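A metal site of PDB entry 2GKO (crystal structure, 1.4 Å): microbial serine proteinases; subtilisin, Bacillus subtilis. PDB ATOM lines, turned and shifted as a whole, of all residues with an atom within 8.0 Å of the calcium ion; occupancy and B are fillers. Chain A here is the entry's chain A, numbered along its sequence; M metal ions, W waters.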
ATOM      1  N   THR A 199       3.686  37.135 -23.594  1.00  0.00           N
ATOM      2  CA  THR A 199       2.406  36.635 -24.071  1.00  0.00           C
ATOM      3  C   THR A 199       1.468  36.484 -22.899  1.00  0.00           C
ATOM      4  O   THR A 199       1.892  36.491 -21.736  1.00  0.00           O
ATOM      5  CB  THR A 199       2.538  35.249 -24.803  1.00  0.00           C
ATOM      6  OG1 THR A 199       2.736  34.196 -23.846  1.00  0.00           O
ATOM      7  CG2 THR A 199       3.776  35.175 -25.732  1.00  0.00           C
ATOM      8  N   VAL A 202      -0.970  30.793 -19.758  1.00  0.00           N
ATOM      9  CA  VAL A 202      -1.939  29.713 -19.542  1.00  0.00           C
ATOM     10  C   VAL A 202      -2.190  29.600 -18.044  1.00  0.00           C
ATOM     11  O   VAL A 202      -1.247  29.572 -17.257  1.00  0.00           O
ATOM     12  CB  VAL A 202      -1.446  28.353 -20.059  1.00  0.00           C
ATOM     13  CG1 VAL A 202      -2.537  27.289 -19.851  1.00  0.00           C
ATOM     14  CG2 VAL A 202      -1.053  28.427 -21.539  1.00  0.00           C
ATOM     15  N   TYR A 217       2.727  20.574 -34.475  1.00  0.00           N
ATOM     16  CA  TYR A 217       1.721  21.377 -35.160  1.00  0.00           C
ATOM     17  C   TYR A 217       0.780  20.508 -35.996  1.00  0.00           C
ATOM     18  O   TYR A 217       0.322  20.912 -37.075  1.00  0.00           O
ATOM     19  CB  TYR A 217       2.383  22.476 -35.996  1.00  0.00           C
ATOM     20  CG  TYR A 217       2.912  23.649 -35.201  1.00  0.00           C
ATOM     21  CD1 TYR A 217       4.288  23.772 -34.946  1.00  0.00           C
ATOM     22  CD2 TYR A 217       2.077  24.659 -34.734  1.00  0.00           C
ATOM     23  CE1 TYR A 217       4.789  24.847 -34.257  1.00  0.00           C
ATOM     24  CE2 TYR A 217       2.577  25.740 -34.038  1.00  0.00           C
ATOM     25  CZ  TYR A 217       3.946  25.830 -33.793  1.00  0.00           C
ATOM     26  OH  TYR A 217       4.489  26.908 -33.114  1.00  0.00           O
ATOM     27  N   SER A 227      -5.510  28.300 -27.503  1.00  0.00           N
ATOM     28  CA  SER A 227      -5.755  28.935 -26.232  1.00  0.00           C
ATOM     29  C   SER A 227      -6.647  30.161 -26.383  1.00  0.00           C
ATOM     30  O   SER A 227      -6.625  30.862 -27.395  1.00  0.00           O
ATOM     31  CB  SER A 227      -4.413  29.321 -25.591  1.00  0.00           C
ATOM     32  OG  SER A 227      -3.585  28.186 -25.413  1.00  0.00           O
ATOM     33  N   ALA A 282      -3.566  30.807 -34.524  1.00  0.00           N
ATOM     34  CA  ALA A 282      -2.984  30.504 -33.226  1.00  0.00           C
ATOM     35  C   ALA A 282      -1.457  30.454 -33.356  1.00  0.00           C
ATOM     36  O   ALA A 282      -0.739  30.982 -32.516  1.00  0.00           O
ATOM     37  CB  ALA A 282      -3.502  29.153 -32.727  1.00  0.00           C
ATOM     38  N   SER A 283      -0.992  29.792 -34.409  1.00  0.00           N
ATOM     39  CA  SER A 283       0.442  29.533 -34.601  1.00  0.00           C
ATOM     40  C   SER A 283       1.275  30.821 -34.705  1.00  0.00           C
ATOM     41  O   SER A 283       2.426  30.845 -34.274  1.00  0.00           O
ATOM     42  CB  SER A 283       0.673  28.666 -35.830  1.00  0.00           C
ATOM     43  OG  SER A 283       0.104  27.387 -35.678  1.00  0.00           O
ATOM     44  N   ASN A 285       0.522  33.485 -33.001  1.00  0.00           N
ATOM     45  CA  ASN A 285       0.527  34.017 -31.644  1.00  0.00           C
ATOM     46  C   ASN A 285       0.897  32.923 -30.661  1.00  0.00           C
ATOM     47  O   ASN A 285       0.118  32.486 -29.833  1.00  0.00           O
ATOM     48  CB  ASN A 285      -0.838  34.617 -31.297  1.00  0.00           C
ATOM     49  CG  ASN A 285      -1.112  35.895 -32.064  1.00  0.00           C
ATOM     50  OD1 ASN A 285      -0.273  36.793 -32.093  1.00  0.00           O
ATOM     51  ND2 ASN A 285      -2.281  35.980 -32.675  1.00  0.00           N
ATOM     52  N   ASP A 286       2.125  32.441 -30.822  1.00  0.00           N
ATOM     53  CA  ASP A 286       2.736  31.462 -29.942  1.00  0.00           C
ATOM     54  C   ASP A 286       2.641  31.895 -28.490  1.00  0.00           C
ATOM     55  O   ASP A 286       3.038  32.995 -28.126  1.00  0.00           O
ATOM     56  CB  ASP A 286       4.212  31.350 -30.357  1.00  0.00           C
ATOM     57  CG  ASP A 286       4.920  30.186 -29.746  1.00  0.00           C
ATOM     58  OD1 ASP A 286       4.340  29.482 -28.877  1.00  0.00           O
ATOM     59  OD2 ASP A 286       6.082  29.887 -30.084  1.00  0.00           O
ATOM     60  N   ILE A 287       2.026  31.056 -27.649  1.00  0.00           N
ATOM     61  CA  ILE A 287       1.930  31.307 -26.230  1.00  0.00           C
ATOM     62  C   ILE A 287       3.176  30.737 -25.566  1.00  0.00           C
ATOM     63  O   ILE A 287       3.555  29.605 -25.817  1.00  0.00           O
ATOM     64  CB  ILE A 287       0.623  30.682 -25.641  1.00  0.00           C
ATOM     65  CG1 ILE A 287      -0.599  31.473 -26.151  1.00  0.00           C
ATOM     66  CG2 ILE A 287       0.679  30.612 -24.107  1.00  0.00           C
ATOM     67  CD1 ILE A 287      -0.751  32.884 -25.588  1.00  0.00           C
ATOM     68  N   LEU A 288       3.793  31.539 -24.703  1.00  0.00           N
ATOM     69  CA  LEU A 288       5.119  31.230 -24.184  1.00  0.00           C
ATOM     70  C   LEU A 288       5.182  31.152 -22.669  1.00  0.00           C
ATOM     71  O   LEU A 288       6.259  31.011 -22.103  1.00  0.00           O
ATOM     72  CB  LEU A 288       6.114  32.309 -24.650  1.00  0.00           C
ATOM     73  CG  LEU A 288       6.297  32.428 -26.152  1.00  0.00           C
ATOM     74  CD1 LEU A 288       7.171  33.661 -26.463  1.00  0.00           C
ATOM     75  CD2 LEU A 288       6.912  31.184 -26.706  1.00  0.00           C
ATOM     76  N   SER A 289       4.037  31.249 -21.989  1.00  0.00           N
ATOM     77  CA  SER A 289       4.085  31.272 -20.533  1.00  0.00           C
ATOM     78  C   SER A 289       2.947  30.468 -19.938  1.00  0.00           C
ATOM     79  O   SER A 289       1.896  30.307 -20.542  1.00  0.00           O
ATOM     80  CB  SER A 289       4.032  32.693 -19.992  1.00  0.00           C
ATOM     81  OG  SER A 289       2.928  33.421 -20.478  1.00  0.00           O
ATOM     82  N   SER A 292       4.643  24.345 -18.476  1.00  0.00           N
ATOM     83  CA  SER A 292       4.843  23.522 -19.683  1.00  0.00           C
ATOM     84  C   SER A 292       4.621  24.289 -20.998  1.00  0.00           C
ATOM     85  O   SER A 292       4.646  23.693 -22.074  1.00  0.00           O
ATOM     86  CB  SER A 292       4.003  22.226 -19.685  1.00  0.00           C
ATOM     87  OG  SER A 292       4.281  21.446 -18.531  1.00  0.00           O
ATOM     88  N   ALA A 293       4.400  25.594 -20.920  1.00  0.00           N
ATOM     89  CA  ALA A 293       4.352  26.399 -22.132  1.00  0.00           C
ATOM     90  C   ALA A 293       5.774  26.750 -22.546  1.00  0.00           C
ATOM     91  O   ALA A 293       6.656  26.935 -21.696  1.00  0.00           O
ATOM     92  CB  ALA A 293       3.546  27.665 -21.899  1.00  0.00           C
ATOM     93  N   GLY A 294       5.991  26.828 -23.846  1.00  0.00           N
ATOM     94  CA  GLY A 294       7.265  27.305 -24.365  1.00  0.00           C
ATOM     95  C   GLY A 294       7.162  27.592 -25.838  1.00  0.00           C
ATOM     96  O   GLY A 294       6.092  27.695 -26.423  1.00  0.00           O
ATOM     97  N   SER A 295       8.321  27.724 -26.474  1.00  0.00           N
ATOM     98  CA  SER A 295       8.351  27.993 -27.893  1.00  0.00           C
ATOM     99  C   SER A 295       7.668  26.888 -28.666  1.00  0.00           C
ATOM    100  O   SER A 295       7.858  25.709 -28.392  1.00  0.00           O
ATOM    101  CB  SER A 295       9.813  28.166 -28.351  1.00  0.00           C
ATOM    102  OG  SER A 295      10.407  29.211 -27.590  1.00  0.00           O
ATOM    103  N   GLY A 296       6.859  27.298 -29.640  1.00  0.00           N
ATOM    104  CA  GLY A 296       6.161  26.379 -30.500  1.00  0.00           C
ATOM    105  C   GLY A 296       4.927  25.732 -29.905  1.00  0.00           C
ATOM    106  O   GLY A 296       4.311  26.229 -28.953  1.00  0.00           O
ATOM    107  N   ASP A 297       4.561  24.611 -30.499  1.00  0.00           N
ATOM    108  CA  ASP A 297       3.357  23.873 -30.163  1.00  0.00           C
ATOM    109  C   ASP A 297       3.632  23.126 -28.845  1.00  0.00           C
ATOM    110  O   ASP A 297       4.524  22.285 -28.805  1.00  0.00           O
ATOM    111  CB  ASP A 297       3.061  22.923 -31.309  1.00  0.00           C
ATOM    112  CG  ASP A 297       1.973  21.936 -31.006  1.00  0.00           C
ATOM    113  OD1 ASP A 297       1.979  20.887 -31.667  1.00  0.00           O
ATOM    114  OD2 ASP A 297       1.098  22.126 -30.119  1.00  0.00           O
ATOM    115  N   ASP A 298       2.884  23.451 -27.787  1.00  0.00           N
ATOM    116  CA  ASP A 298       3.157  22.868 -26.461  1.00  0.00           C
ATOM    117  C   ASP A 298       1.894  22.326 -25.806  1.00  0.00           C
ATOM    118  O   ASP A 298       0.776  22.578 -26.263  1.00  0.00           O
ATOM    119  CB  ASP A 298       3.916  23.845 -25.564  1.00  0.00           C
ATOM    120  CG  ASP A 298       3.167  25.122 -25.318  1.00  0.00           C
ATOM    121  OD1 ASP A 298       2.092  25.027 -24.705  1.00  0.00           O
ATOM    122  OD2 ASP A 298       3.545  26.252 -25.665  1.00  0.00           O
ATOM    123  N   ILE A 299       2.082  21.555 -24.747  1.00  0.00           N
ATOM    124  CA  ILE A 299       0.948  20.859 -24.130  1.00  0.00           C
ATOM    125  C   ILE A 299       0.049  21.794 -23.302  1.00  0.00           C
ATOM    126  O   ILE A 299      -1.075  21.419 -22.972  1.00  0.00           O
ATOM    127  CB  ILE A 299       1.395  19.660 -23.230  1.00  0.00           C
ATOM    128  CG1 ILE A 299       2.265  20.142 -22.080  1.00  0.00           C
ATOM    129  CG2 ILE A 299       2.090  18.598 -24.077  1.00  0.00           C
ATOM    130  CD1 ILE A 299       2.653  19.022 -21.126  1.00  0.00           C
ATOM    131  N   ALA A 300       0.553  22.960 -22.958  1.00  0.00           N
ATOM    132  CA  ALA A 300      -0.220  23.930 -22.187  1.00  0.00           C
ATOM    133  C   ALA A 300      -1.186  24.726 -23.042  1.00  0.00           C
ATOM    134  O   ALA A 300      -2.329  24.961 -22.652  1.00  0.00           O
ATOM    135  CB  ALA A 300       0.689  24.867 -21.465  1.00  0.00           C
ATOM    136  N   SER A 301      -0.724  25.123 -24.221  1.00  0.00           N
ATOM    137  CA  SER A 301      -1.405  26.108 -25.033  1.00  0.00           C
ATOM    138  C   SER A 301      -1.669  25.681 -26.479  1.00  0.00           C
ATOM    139  O   SER A 301      -2.247  26.442 -27.237  1.00  0.00           O
ATOM    140  CB  SER A 301      -0.603  27.414 -25.019  1.00  0.00           C
ATOM    141  OG  SER A 301       0.685  27.215 -25.591  1.00  0.00           O
ATOM    142  N   GLY A 302      -1.290  24.452 -26.845  1.00  0.00           N
ATOM    143  CA  GLY A 302      -1.348  24.012 -28.217  1.00  0.00           C
ATOM    144  C   GLY A 302      -0.561  24.962 -29.125  1.00  0.00           C
ATOM    145  O   GLY A 302       0.553  25.386 -28.770  1.00  0.00           O
ATOM    146  N   PHE A 303      -1.147  25.336 -30.253  1.00  0.00           N
ATOM    147  CA  PHE A 303      -0.444  26.111 -31.285  1.00  0.00           C
ATOM    148  C   PHE A 303      -0.279  27.572 -30.904  1.00  0.00           C
ATOM    149  O   PHE A 303       0.622  28.269 -31.418  1.00  0.00           O
ATOM    150  CB  PHE A 303      -1.190  26.052 -32.619  1.00  0.00           C
ATOM    151  CG  PHE A 303      -1.313  24.674 -33.245  1.00  0.00           C
ATOM    152  CD1 PHE A 303      -0.905  23.494 -32.596  1.00  0.00           C
ATOM    153  CD2 PHE A 303      -1.855  24.574 -34.521  1.00  0.00           C
ATOM    154  CE1 PHE A 303      -1.063  22.271 -33.182  1.00  0.00           C
ATOM    155  CE2 PHE A 303      -2.008  23.358 -35.113  1.00  0.00           C
ATOM    156  CZ  PHE A 303      -1.604  22.195 -34.467  1.00  0.00           C
ATOM    157  N   GLY A 304      -1.146  28.059 -30.025  1.00  0.00           N
ATOM    158  CA  GLY A 304      -1.162  29.442 -29.582  1.00  0.00           C
ATOM    159  C   GLY A 304      -2.548  30.015 -29.395  1.00  0.00           C
ATOM    160  O   GLY A 304      -3.522  29.286 -29.172  1.00  0.00           O
ATOM    161  N   PHE A 305      -2.637  31.334 -29.536  1.00  0.00           N
ATOM    162  CA  PHE A 305      -3.835  32.102 -29.229  1.00  0.00           C
ATOM    163  C   PHE A 305      -4.365  32.733 -30.530  1.00  0.00           C
ATOM    164  O   PHE A 305      -3.855  33.768 -30.988  1.00  0.00           O
ATOM    165  CB  PHE A 305      -3.440  33.185 -28.197  1.00  0.00           C
ATOM    166  CG  PHE A 305      -4.565  34.116 -27.756  1.00  0.00           C
ATOM    167  CD1 PHE A 305      -4.286  35.209 -26.951  1.00  0.00           C
ATOM    168  CD2 PHE A 305      -5.883  33.898 -28.121  1.00  0.00           C
ATOM    169  CE1 PHE A 305      -5.271  36.069 -26.530  1.00  0.00           C
ATOM    170  CE2 PHE A 305      -6.878  34.769 -27.698  1.00  0.00           C
ATOM    171  CZ  PHE A 305      -6.591  35.824 -26.911  1.00  0.00           C
HETATM  172 CA    CA M   1       4.007  27.835 -27.292  1.00  0.00          CA
HETATM  173  O   HOH W   1       1.668  27.946 -27.948  1.00  0.00           O
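OD1 of Asp 298 is in hydrogen-bond range of OG of Ser 301, at 2.7 Å. O of Ser 301 is in hydrogen-bond range of OG of Ser 227, at 2.9 Å. The backbone NH (N) of Ala 300 is in hydrogen-bond range of the side-chain carboxylate (OD1) of Asp 298, at 3.1 Å.
Water W1 lies within hydrogen-bond range of the side-chain hydroxyl of Ser 301 (2.7 Å), the backbone carbonyl oxygen of Gly 302 (2.9 Å), the backbone NH of Ile 287 (3.1 Å) and the backbone NH of Gly 304 (3.5 Å).
The backbone carbonyl oxygen (O) of Gly 294 binds the calcium ion, at 2.3 Å. OD1 of Asp 286 binds the calcium ion (2.3 Å). The calcium ion is bound by OD2 of Asp 298 (2.3 Å). O of Gly 296 is bound to the calcium ion (2.3 Å). The calcium ion is bound by O of Ile 287, 2.3 Å away. Water W1 is bound to the calcium ion (2.4 Å). The calcium ion has six donor atoms within binding distance.
OG of Ser 301 touches the calcium ion (3.8 Å).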
